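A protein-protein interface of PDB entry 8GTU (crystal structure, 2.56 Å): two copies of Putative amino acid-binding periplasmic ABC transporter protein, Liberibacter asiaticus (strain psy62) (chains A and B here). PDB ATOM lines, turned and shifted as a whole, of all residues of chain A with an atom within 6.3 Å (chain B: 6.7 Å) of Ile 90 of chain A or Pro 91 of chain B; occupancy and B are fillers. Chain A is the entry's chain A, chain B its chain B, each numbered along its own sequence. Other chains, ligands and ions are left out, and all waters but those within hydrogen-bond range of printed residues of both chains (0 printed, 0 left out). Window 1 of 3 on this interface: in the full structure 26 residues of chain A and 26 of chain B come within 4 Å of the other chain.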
ATOM      1  N   ILE A  78      25.657  -6.703   0.672  1.00  0.00           N
ATOM      2  CA  ILE A  78      26.228  -8.027   0.456  1.00  0.00           C
ATOM      3  C   ILE A  78      26.276  -8.311  -1.053  1.00  0.00           C
ATOM      4  O   ILE A  78      25.269  -8.200  -1.758  1.00  0.00           O
ATOM      5  CB  ILE A  78      25.443  -9.098   1.252  1.00  0.00           C
ATOM      6  CG1 ILE A  78      25.560  -8.908   2.775  1.00  0.00           C
ATOM      7  CG2 ILE A  78      25.857 -10.502   0.843  1.00  0.00           C
ATOM      8  CD1 ILE A  78      24.664  -9.820   3.604  1.00  0.00           C
ATOM      9  N   PHE A  88      30.623 -11.078   6.689  1.00  0.00           N
ATOM     10  CA  PHE A  88      29.463 -10.224   6.947  1.00  0.00           C
ATOM     11  C   PHE A  88      28.657 -10.748   8.131  1.00  0.00           C
ATOM     12  O   PHE A  88      28.583 -11.959   8.339  1.00  0.00           O
ATOM     13  CB  PHE A  88      28.477 -10.234   5.783  1.00  0.00           C
ATOM     14  CG  PHE A  88      28.878  -9.441   4.573  1.00  0.00           C
ATOM     15  CD1 PHE A  88      28.702  -8.069   4.543  1.00  0.00           C
ATOM     16  CD2 PHE A  88      29.375 -10.071   3.439  1.00  0.00           C
ATOM     17  CE1 PHE A  88      29.026  -7.337   3.408  1.00  0.00           C
ATOM     18  CE2 PHE A  88      29.697  -9.331   2.309  1.00  0.00           C
ATOM     19  CZ  PHE A  88      29.531  -7.963   2.300  1.00  0.00           C
ATOM     20  N   SER A  89      28.022  -9.833   8.868  1.00  0.00           N
ATOM     21  CA  SER A  89      27.012 -10.219   9.836  1.00  0.00           C
ATOM     22  C   SER A  89      25.734 -10.674   9.127  1.00  0.00           C
ATOM     23  O   SER A  89      25.611 -10.558   7.913  1.00  0.00           O
ATOM     24  CB  SER A  89      26.752  -9.101  10.805  1.00  0.00           C
ATOM     25  OG  SER A  89      26.164  -7.989  10.149  1.00  0.00           O
ATOM     26  N   ILE A  90      24.813 -11.287   9.873  1.00  0.00           N
ATOM     27  CA  ILE A  90      23.438 -11.454   9.432  1.00  0.00           C
ATOM     28  C   ILE A  90      22.929 -10.083   8.952  1.00  0.00           C
ATOM     29  O   ILE A  90      23.271  -9.043   9.538  1.00  0.00           O
ATOM     30  CB  ILE A  90      22.606 -12.044  10.594  1.00  0.00           C
ATOM     31  CG1 ILE A  90      21.198 -12.495  10.182  1.00  0.00           C
ATOM     32  CG2 ILE A  90      22.581 -11.107  11.798  1.00  0.00           C
ATOM     33  CD1 ILE A  90      20.527 -13.448  11.173  1.00  0.00           C
ATOM     34  N   PRO A  91      22.194 -10.012   7.810  1.00  0.00           N
ATOM     35  CA  PRO A  91      21.653  -8.736   7.334  1.00  0.00           C
ATOM     36  C   PRO A  91      20.840  -8.053   8.437  1.00  0.00           C
ATOM     37  O   PRO A  91      20.103  -8.727   9.139  1.00  0.00           O
ATOM     38  CB  PRO A  91      20.717  -9.144   6.185  1.00  0.00           C
ATOM     39  CG  PRO A  91      21.288 -10.453   5.688  1.00  0.00           C
ATOM     40  CD  PRO A  91      21.912 -11.128   6.889  1.00  0.00           C
ATOM     41  N   TYR A  92      20.974  -6.735   8.602  1.00  0.00           N
ATOM     42  CA  TYR A  92      20.174  -6.049   9.610  1.00  0.00           C
ATOM     43  C   TYR A  92      19.195  -5.051   8.986  1.00  0.00           C
ATOM     44  O   TYR A  92      18.376  -4.500   9.691  1.00  0.00           O
ATOM     45  CB  TYR A  92      21.034  -5.360  10.673  1.00  0.00           C
ATOM     46  CG  TYR A  92      21.931  -4.262  10.157  1.00  0.00           C
ATOM     47  CD1 TYR A  92      21.469  -2.969   9.914  1.00  0.00           C
ATOM     48  CD2 TYR A  92      23.266  -4.515   9.929  1.00  0.00           C
ATOM     49  CE1 TYR A  92      22.315  -1.965   9.456  1.00  0.00           C
ATOM     50  CE2 TYR A  92      24.122  -3.524   9.484  1.00  0.00           C
ATOM     51  CZ  TYR A  92      23.651  -2.252   9.239  1.00  0.00           C
ATOM     52  OH  TYR A  92      24.534  -1.331   8.756  1.00  0.00           O
ATOM     53  N   ILE A  93      19.306  -4.789   7.683  1.00  0.00           N
ATOM     54  CA  ILE A  93      18.409  -3.889   6.978  1.00  0.00           C
ATOM     55  C   ILE A  93      18.427  -4.309   5.505  1.00  0.00           C
ATOM     56  O   ILE A  93      19.172  -5.218   5.115  1.00  0.00           O
ATOM     57  CB  ILE A  93      18.822  -2.416   7.224  1.00  0.00           C
ATOM     58  CG1 ILE A  93      17.804  -1.416   6.688  1.00  0.00           C
ATOM     59  CG2 ILE A  93      20.200  -2.097   6.683  1.00  0.00           C
ATOM     60  CD1 ILE A  93      16.619  -1.267   7.563  1.00  0.00           C
ATOM     61  N   VAL A 192      21.735  -5.730   3.633  1.00  0.00           N
ATOM     62  CA  VAL A 192      22.794  -4.824   4.063  1.00  0.00           C
ATOM     63  C   VAL A 192      23.309  -5.326   5.407  1.00  0.00           C
ATOM     64  O   VAL A 192      22.515  -5.670   6.267  1.00  0.00           O
ATOM     65  CB  VAL A 192      22.225  -3.404   4.209  1.00  0.00           C
ATOM     66  CG1 VAL A 192      23.163  -2.504   4.985  1.00  0.00           C
ATOM     67  CG2 VAL A 192      21.812  -2.796   2.869  1.00  0.00           C
ATOM     68  N   ALA A 193      24.625  -5.345   5.609  1.00  0.00           N
ATOM     69  CA  ALA A 193      25.169  -5.935   6.822  1.00  0.00           C
ATOM     70  C   ALA A 193      26.383  -5.126   7.267  1.00  0.00           C
ATOM     71  O   ALA A 193      26.790  -4.190   6.584  1.00  0.00           O
ATOM     72  CB  ALA A 193      25.528  -7.379   6.555  1.00  0.00           C
ATOM     73  N   PHE A 194      26.926  -5.477   8.437  1.00  0.00           N
ATOM     74  CA  PHE A 194      28.242  -5.015   8.858  1.00  0.00           C
ATOM     75  C   PHE A 194      29.283  -5.859   8.135  1.00  0.00           C
ATOM     76  O   PHE A 194      29.095  -7.062   7.958  1.00  0.00           O
ATOM     77  CB  PHE A 194      28.419  -5.155  10.379  1.00  0.00           C
ATOM     78  CG  PHE A 194      27.410  -4.397  11.198  1.00  0.00           C
ATOM     79  CD1 PHE A 194      27.361  -3.021  11.149  1.00  0.00           C
ATOM     80  CD2 PHE A 194      26.486  -5.056  11.992  1.00  0.00           C
ATOM     81  CE1 PHE A 194      26.424  -2.310  11.887  1.00  0.00           C
ATOM     82  CE2 PHE A 194      25.550  -4.348  12.740  1.00  0.00           C
ATOM     83  CZ  PHE A 194      25.513  -2.975  12.673  1.00  0.00           C
ATOM     84  N   THR A 204      32.408 -11.887  14.449  1.00  0.00           N
ATOM     85  CA  THR A 204      31.251 -11.989  13.569  1.00  0.00           C
ATOM     86  C   THR A 204      30.093 -12.676  14.297  1.00  0.00           C
ATOM     87  O   THR A 204      28.968 -12.175  14.280  1.00  0.00           O
ATOM     88  CB  THR A 204      31.637 -12.593  12.210  1.00  0.00           C
ATOM     89  OG1 THR A 204      32.653 -11.735  11.684  1.00  0.00           O
ATOM     90  CG2 THR A 204      30.472 -12.726  11.243  1.00  0.00           C
ATOM     91  N   ILE A 207      28.560 -10.291  17.124  1.00  0.00           N
ATOM     92  CA  ILE A 207      27.670  -9.268  16.601  1.00  0.00           C
ATOM     93  C   ILE A 207      26.309  -9.914  16.293  1.00  0.00           C
ATOM     94  O   ILE A 207      25.255  -9.356  16.620  1.00  0.00           O
ATOM     95  CB  ILE A 207      28.313  -8.544  15.390  1.00  0.00           C
ATOM     96  CG1 ILE A 207      29.608  -7.811  15.762  1.00  0.00           C
ATOM     97  CG2 ILE A 207      27.327  -7.615  14.684  1.00  0.00           C
ATOM     98  CD1 ILE A 207      30.328  -7.177  14.588  1.00  0.00           C
ATOM     99  N   ASN A 208      26.346 -11.129  15.728  1.00  0.00           N
ATOM    100  CA  ASN A 208      25.161 -11.830  15.271  1.00  0.00           C
ATOM    101  C   ASN A 208      24.288 -12.235  16.453  1.00  0.00           C
ATOM    102  O   ASN A 208      23.063 -12.138  16.404  1.00  0.00           O
ATOM    103  CB  ASN A 208      25.513 -13.071  14.446  1.00  0.00           C
ATOM    104  CG  ASN A 208      26.063 -12.738  13.081  1.00  0.00           C
ATOM    105  OD1 ASN A 208      25.952 -11.605  12.635  1.00  0.00           O
ATOM    106  ND2 ASN A 208      26.678 -13.707  12.425  1.00  0.00           N
ATOM    107  N   LEU A 211      22.836  -8.987  17.723  1.00  0.00           N
ATOM    108  CA  LEU A 211      21.781  -8.499  16.850  1.00  0.00           C
ATOM    109  C   LEU A 211      20.486  -9.274  17.079  1.00  0.00           C
ATOM    110  O   LEU A 211      19.398  -8.708  17.003  1.00  0.00           O
ATOM    111  CB  LEU A 211      22.222  -8.580  15.386  1.00  0.00           C
ATOM    112  CG  LEU A 211      23.085  -7.407  14.928  1.00  0.00           C
ATOM    113  CD1 LEU A 211      23.652  -7.671  13.545  1.00  0.00           C
ATOM    114  CD2 LEU A 211      22.252  -6.139  14.930  1.00  0.00           C
ATOM    115  N   CYS A 212      20.600 -10.577  17.343  1.00  0.00           N
ATOM    116  CA  CYS A 212      19.394 -11.365  17.498  1.00  0.00           C
ATOM    117  C   CYS A 212      18.725 -11.039  18.828  1.00  0.00           C
ATOM    118  O   CYS A 212      17.501 -10.986  18.905  1.00  0.00           O
ATOM    119  CB  CYS A 212      19.639 -12.845  17.257  1.00  0.00           C
ATOM    120  SG  CYS A 212      19.474 -13.264  15.501  1.00  0.00           S
ATOM    121  N   PRO A 237      13.899 -10.342   8.641  1.00  0.00           N
ATOM    122  CA  PRO A 237      13.111 -11.152   9.560  1.00  0.00           C
ATOM    123  C   PRO A 237      13.733 -11.107  10.950  1.00  0.00           C
ATOM    124  O   PRO A 237      14.918 -10.836  11.098  1.00  0.00           O
ATOM    125  CB  PRO A 237      13.195 -12.541   8.929  1.00  0.00           C
ATOM    126  CG  PRO A 237      14.461 -12.518   8.124  1.00  0.00           C
ATOM    127  CD  PRO A 237      14.524 -11.125   7.569  1.00  0.00           C
ATOM    128  N   GLY A 238      12.911 -11.346  11.972  1.00  0.00           N
ATOM    129  CA  GLY A 238      13.400 -11.332  13.345  1.00  0.00           C
ATOM    130  C   GLY A 238      14.204 -12.585  13.695  1.00  0.00           C
ATOM    131  O   GLY A 238      14.705 -13.277  12.807  1.00  0.00           O
ATOM    132  N   CYS A 239      14.385 -12.845  14.997  1.00  0.00           N
ATOM    133  CA  CYS A 239      14.999 -14.077  15.474  1.00  0.00           C
ATOM    134  C   CYS A 239      13.977 -14.755  16.388  1.00  0.00           C
ATOM    135  O   CYS A 239      12.962 -14.148  16.702  1.00  0.00           O
ATOM    136  CB  CYS A 239      16.370 -13.816  16.105  1.00  0.00           C
ATOM    137  SG  CYS A 239      17.498 -12.867  15.029  1.00  0.00           S
ATOM    138  N   ILE B  78      17.115 -19.473  13.483  1.00  0.00           N
ATOM    139  CA  ILE B  78      18.195 -18.765  14.148  1.00  0.00           C
ATOM    140  C   ILE B  78      17.707 -18.262  15.515  1.00  0.00           C
ATOM    141  O   ILE B  78      16.713 -17.554  15.630  1.00  0.00           O
ATOM    142  CB  ILE B  78      18.723 -17.626  13.241  1.00  0.00           C
ATOM    143  CG1 ILE B  78      19.296 -18.127  11.907  1.00  0.00           C
ATOM    144  CG2 ILE B  78      19.708 -16.751  13.985  1.00  0.00           C
ATOM    145  CD1 ILE B  78      19.743 -17.046  10.944  1.00  0.00           C
ATOM    146  N   GLN B  83      23.094 -19.405  17.916  1.00  0.00           N
ATOM    147  CA  GLN B  83      24.092 -18.552  17.288  1.00  0.00           C
ATOM    148  C   GLN B  83      25.411 -18.634  18.054  1.00  0.00           C
ATOM    149  O   GLN B  83      26.492 -18.578  17.474  1.00  0.00           O
ATOM    150  CB  GLN B  83      23.599 -17.109  17.166  1.00  0.00           C
ATOM    151  CG  GLN B  83      23.108 -16.771  15.772  1.00  0.00           C
ATOM    152  CD  GLN B  83      22.568 -15.367  15.656  1.00  0.00           C
ATOM    153  OE1 GLN B  83      22.224 -14.726  16.648  1.00  0.00           O
ATOM    154  NE2 GLN B  83      22.487 -14.881  14.425  1.00  0.00           N
ATOM    155  N   PHE B  88      25.637 -20.394  11.190  1.00  0.00           N
ATOM    156  CA  PHE B  88      24.498 -20.342  10.287  1.00  0.00           C
ATOM    157  C   PHE B  88      24.878 -19.673   8.971  1.00  0.00           C
ATOM    158  O   PHE B  88      25.706 -18.773   8.950  1.00  0.00           O
ATOM    159  CB  PHE B  88      23.392 -19.463  10.873  1.00  0.00           C
ATOM    160  CG  PHE B  88      22.555 -20.084  11.956  1.00  0.00           C
ATOM    161  CD1 PHE B  88      21.536 -20.966  11.649  1.00  0.00           C
ATOM    162  CD2 PHE B  88      22.781 -19.765  13.289  1.00  0.00           C
ATOM    163  CE1 PHE B  88      20.778 -21.542  12.654  1.00  0.00           C
ATOM    164  CE2 PHE B  88      22.007 -20.322  14.292  1.00  0.00           C
ATOM    165  CZ  PHE B  88      21.012 -21.215  13.976  1.00  0.00           C
ATOM    166  N   SER B  89      24.210 -20.070   7.887  1.00  0.00           N
ATOM    167  CA  SER B  89      24.240 -19.292   6.657  1.00  0.00           C
ATOM    168  C   SER B  89      23.433 -17.997   6.812  1.00  0.00           C
ATOM    169  O   SER B  89      22.731 -17.809   7.800  1.00  0.00           O
ATOM    170  CB  SER B  89      23.776 -20.117   5.479  1.00  0.00           C
ATOM    171  OG  SER B  89      22.400 -20.436   5.592  1.00  0.00           O
ATOM    172  N   ILE B  90      23.569 -17.072   5.851  1.00  0.00           N
ATOM    173  CA  ILE B  90      22.594 -16.003   5.663  1.00  0.00           C
ATOM    174  C   ILE B  90      21.190 -16.631   5.671  1.00  0.00           C
ATOM    175  O   ILE B  90      21.009 -17.754   5.170  1.00  0.00           O
ATOM    176  CB  ILE B  90      22.933 -15.258   4.355  1.00  0.00           C
ATOM    177  CG1 ILE B  90      22.191 -13.927   4.197  1.00  0.00           C
ATOM    178  CG2 ILE B  90      22.778 -16.163   3.142  1.00  0.00           C
ATOM    179  CD1 ILE B  90      22.689 -13.040   3.037  1.00  0.00           C
ATOM    180  N   PRO B  91      20.166 -16.007   6.304  1.00  0.00           N
ATOM    181  CA  PRO B  91      18.800 -16.542   6.241  1.00  0.00           C
ATOM    182  C   PRO B  91      18.367 -16.758   4.788  1.00  0.00           C
ATOM    183  O   PRO B  91      18.692 -15.943   3.932  1.00  0.00           O
ATOM    184  CB  PRO B  91      17.936 -15.443   6.875  1.00  0.00           C
ATOM    185  CG  PRO B  91      18.895 -14.611   7.725  1.00  0.00           C
ATOM    186  CD  PRO B  91      20.284 -14.816   7.157  1.00  0.00           C
ATOM    187  N   TYR B  92      17.664 -17.859   4.491  1.00  0.00           N
ATOM    188  CA  TYR B  92      17.123 -18.035   3.152  1.00  0.00           C
ATOM    189  C   TYR B  92      15.594 -18.049   3.153  1.00  0.00           C
ATOM    190  O   TYR B  92      15.004 -18.053   2.078  1.00  0.00           O
ATOM    191  CB  TYR B  92      17.694 -19.274   2.448  1.00  0.00           C
ATOM    192  CG  TYR B  92      17.373 -20.593   3.103  1.00  0.00           C
ATOM    193  CD1 TYR B  92      16.154 -21.233   2.876  1.00  0.00           C
ATOM    194  CD2 TYR B  92      18.291 -21.203   3.960  1.00  0.00           C
ATOM    195  CE1 TYR B  92      15.870 -22.457   3.468  1.00  0.00           C
ATOM    196  CE2 TYR B  92      18.010 -22.411   4.579  1.00  0.00           C
ATOM    197  CZ  TYR B  92      16.798 -23.026   4.326  1.00  0.00           C
ATOM    198  OH  TYR B  92      16.513 -24.203   4.941  1.00  0.00           O
ATOM    199  N   ILE B  93      14.955 -18.110   4.333  1.00  0.00           N
ATOM    200  CA  ILE B  93      13.503 -18.054   4.399  1.00  0.00           C
ATOM    201  C   ILE B  93      13.063 -17.527   5.763  1.00  0.00           C
ATOM    202  O   ILE B  93      13.885 -17.334   6.656  1.00  0.00           O
ATOM    203  CB  ILE B  93      12.864 -19.407   3.999  1.00  0.00           C
ATOM    204  CG1 ILE B  93      11.359 -19.260   3.762  1.00  0.00           C
ATOM    205  CG2 ILE B  93      13.219 -20.530   4.973  1.00  0.00           C
ATOM    206  CD1 ILE B  93      10.844 -20.094   2.650  1.00  0.00           C
ATOM    207  N   ALA B  94      11.763 -17.258   5.912  1.00  0.00           N
ATOM    208  CA  ALA B  94      11.254 -16.846   7.204  1.00  0.00           C
ATOM    209  C   ALA B  94       9.895 -17.478   7.414  1.00  0.00           C
ATOM    210  O   ALA B  94       9.137 -17.607   6.471  1.00  0.00           O
ATOM    211  CB  ALA B  94      11.184 -15.350   7.307  1.00  0.00           C
ATOM    212  N   ALA B 191      13.792 -15.639  10.969  1.00  0.00           N
ATOM    213  CA  ALA B 191      14.812 -16.075  10.026  1.00  0.00           C
ATOM    214  C   ALA B 191      15.133 -17.567  10.196  1.00  0.00           C
ATOM    215  O   ALA B 191      15.269 -18.070  11.307  1.00  0.00           O
ATOM    216  CB  ALA B 191      16.056 -15.223  10.176  1.00  0.00           C
ATOM    217  N   VAL B 192      15.296 -18.254   9.057  1.00  0.00           N
ATOM    218  CA  VAL B 192      15.569 -19.678   8.992  1.00  0.00           C
ATOM    219  C   VAL B 192      16.798 -19.857   8.113  1.00  0.00           C
ATOM    220  O   VAL B 192      16.900 -19.203   7.080  1.00  0.00           O
ATOM    221  CB  VAL B 192      14.360 -20.380   8.355  1.00  0.00           C
ATOM    222  CG1 VAL B 192      14.707 -21.779   7.887  1.00  0.00           C
ATOM    223  CG2 VAL B 192      13.121 -20.338   9.241  1.00  0.00           C
ATOM    224  N   ALA B 193      17.732 -20.723   8.507  1.00  0.00           N
ATOM    225  CA  ALA B 193      18.998 -20.803   7.786  1.00  0.00           C
ATOM    226  C   ALA B 193      19.509 -22.235   7.841  1.00  0.00           C
ATOM    227  O   ALA B 193      18.902 -23.065   8.523  1.00  0.00           O
ATOM    228  CB  ALA B 193      20.022 -19.853   8.366  1.00  0.00           C
ATOM    229  N   PHE B 194      20.599 -22.504   7.102  1.00  0.00           N
ATOM    230  CA  PHE B 194      21.324 -23.762   7.230  1.00  0.00           C
ATOM    231  C   PHE B 194      22.191 -23.695   8.480  1.00  0.00           C
ATOM    232  O   PHE B 194      22.756 -22.653   8.760  1.00  0.00           O
ATOM    233  CB  PHE B 194      22.202 -24.029   5.996  1.00  0.00           C
ATOM    234  CG  PHE B 194      21.433 -24.151   4.707  1.00  0.00           C
ATOM    235  CD1 PHE B 194      20.489 -25.150   4.522  1.00  0.00           C
ATOM    236  CD2 PHE B 194      21.618 -23.226   3.695  1.00  0.00           C
ATOM    237  CE1 PHE B 194      19.789 -25.247   3.334  1.00  0.00           C
ATOM    238  CE2 PHE B 194      20.899 -23.311   2.511  1.00  0.00           C
ATOM    239  CZ  PHE B 194      19.985 -24.320   2.333  1.00  0.00           C
ATOM    240  N   ASN B 208      27.121 -19.383   1.353  1.00  0.00           N
ATOM    241  CA  ASN B 208      26.638 -18.012   1.314  1.00  0.00           C
ATOM    242  C   ASN B 208      26.868 -17.403  -0.061  1.00  0.00           C
ATOM    243  O   ASN B 208      26.010 -16.695  -0.579  1.00  0.00           O
ATOM    244  CB  ASN B 208      27.288 -17.167   2.408  1.00  0.00           C
ATOM    245  CG  ASN B 208      26.728 -17.483   3.779  1.00  0.00           C
ATOM    246  OD1 ASN B 208      25.652 -18.070   3.890  1.00  0.00           O
ATOM    247  ND2 ASN B 208      27.438 -17.088   4.822  1.00  0.00           N
ATOM    248  N   LEU B 211      24.381 -19.158  -2.290  1.00  0.00           N
ATOM    249  CA  LEU B 211      23.019 -18.688  -2.068  1.00  0.00           C
ATOM    250  C   LEU B 211      22.809 -17.328  -2.727  1.00  0.00           C
ATOM    251  O   LEU B 211      21.729 -17.037  -3.230  1.00  0.00           O
ATOM    252  CB  LEU B 211      22.727 -18.617  -0.570  1.00  0.00           C
ATOM    253  CG  LEU B 211      22.359 -19.946   0.083  1.00  0.00           C
ATOM    254  CD1 LEU B 211      22.212 -19.758   1.577  1.00  0.00           C
ATOM    255  CD2 LEU B 211      21.094 -20.555  -0.523  1.00  0.00           C
ATOM    256  N   HIS B 215      20.077 -16.422  -5.519  1.00  0.00           N
ATOM    257  CA  HIS B 215      19.227 -15.234  -5.536  1.00  0.00           C
ATOM    258  C   HIS B 215      19.309 -14.561  -6.909  1.00  0.00           C
ATOM    259  O   HIS B 215      18.279 -14.342  -7.540  1.00  0.00           O
ATOM    260  CB  HIS B 215      19.443 -14.265  -4.358  1.00  0.00           C
ATOM    261  CG  HIS B 215      18.756 -14.687  -3.078  1.00  0.00           C
ATOM    262  ND1 HIS B 215      17.414 -14.485  -2.802  1.00  0.00           N
ATOM    263  CD2 HIS B 215      19.263 -15.323  -1.985  1.00  0.00           C
ATOM    264  CE1 HIS B 215      17.121 -14.987  -1.606  1.00  0.00           C
ATOM    265  NE2 HIS B 215      18.235 -15.494  -1.088  1.00  0.00           N
ATOM    266  N   VAL B 236      13.332 -13.531   2.158  1.00  0.00           N
ATOM    267  CA  VAL B 236      14.381 -12.699   2.724  1.00  0.00           C
ATOM    268  C   VAL B 236      14.879 -11.723   1.660  1.00  0.00           C
ATOM    269  O   VAL B 236      14.592 -11.904   0.479  1.00  0.00           O
ATOM    270  CB  VAL B 236      15.505 -13.588   3.268  1.00  0.00           C
ATOM    271  CG1 VAL B 236      14.999 -14.388   4.443  1.00  0.00           C
ATOM    272  CG2 VAL B 236      16.042 -14.509   2.186  1.00  0.00           C
ATOM    273  N   PRO B 237      15.607 -10.645   2.028  1.00  0.00           N
ATOM    274  CA  PRO B 237      16.126  -9.712   1.030  1.00  0.00           C
ATOM    275  C   PRO B 237      17.195 -10.396   0.188  1.00  0.00           C
ATOM    276  O   PRO B 237      17.890 -11.304   0.653  1.00  0.00           O
ATOM    277  CB  PRO B 237      16.709  -8.553   1.847  1.00  0.00           C
ATOM    278  CG  PRO B 237      16.987  -9.172   3.200  1.00  0.00           C
ATOM    279  CD  PRO B 237      15.930 -10.240   3.402  1.00  0.00           C
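The side-chain amide oxygen (OE1) of Gln 83 of chain B lies close to the backbone carbonyl oxygen (O) of Asn 208 of chain A (2.7 Å). The side-chain sulfur (SG) of Cys 212 of chain A sits close to the side-chain amide oxygen (OE1) of Gln 83 of chain B (3.3 Å). The backbone NH (N) of Ala 191 of chain B lies within hydrogen-bond range of the backbone carbonyl oxygen (O) of Gly 238 of chain A (3.1 Å).
The side-chain amide oxygen (OD1) of Asn 208 of chain A is in hydrogen-bond range of the backbone NH (N) of Ile 90 of chain A (3.0 Å). The backbone carbonyl oxygen of Thr 204 of chain A lies close to the side-chain amide nitrogen of Asn 208 of chain A (3.3 Å). SG of Cys 212 of chain A is disulfide-bonded to SG of Cys 239 of chain A (2.1 Å). The backbone NH (N) of Ile 78 of chain B lies within hydrogen-bond range of the backbone carbonyl oxygen (O) of Ala 191 of chain B, 3.2 Å away. The backbone NH of Ile 90 of chain B sits at hydrogen-bond distance from the side-chain amide oxygen of Asn 208 of chain B, at 3.0 Å.
Ile 90 of chain B touches Ile 78 of chain A (CD1 to CD1, 3.8 Å). Ile 90 of chain A touches Ile 78 of chain B (CD1 to CD1, 3.7 Å). CD of Pro 91 of chain B touches CG1 of Ile 90 of chain A, at 3.9 Å. CG of Pro 91 of chain A touches CG1 of Ile 90 of chain B, 3.9 Å away. Cys 212 of chain A touches Ile 78 of chain B. Pro 237 of chain A touches Ala 94 of chain B (CB to CB, 3.8 Å). Pro 237 of chain A touches Ala 191 of chain B. Cys 239 of chain A touches Ile 78 of chain B (CB to O, 3.8 Å).
Ile 90 of chain A touches two residues of chain B. Of chain A, only Ile 90 comes within 4 Å of Pro 91 of chain B. Of the printed residues of chain A, Ala 94 of chain B touches Pro 237. Printed residues of chain B within 4 Å of Cys 212 of chain A: Ile 78 and Gln 83. Printed residues of chain B within 4 Å of Asn 208 of chain A: Gln 83 (2.7 Å). Ala 193 of chain A touches none of the printed residues of chain B. Phe 194 of chain A touches none of the printed residues of chain B. The nearest residue of chain B that does not touch Ile 90 of chain A is Gln 83 of chain B (4.1 Å). The nearest printed residue of chain A that does not touch Ala 191 of chain B is Ile 90 of chain A (4.9 Å).
Hydrophobic or aromatic side chains of chain A within 4 Å of the printed part of chain B: Ile 78, Ile 90, Pro 91 and Pro 237. Among the printed residues, 11 pairs touch across the chains.
Ile 78 of chain A touches Ile 90 of chain B, and with the chains exchanged Ile 90 of chain A touches Ile 78 of chain B. Ile 90 of chain A touches Pro 91 of chain B, and with the chains exchanged Pro 91 of chain A touches Ile 90 of chain B. Of the 11 pairs that touch across the chains among the printed residues, 4 have their exchanged pair printed and touching as well.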
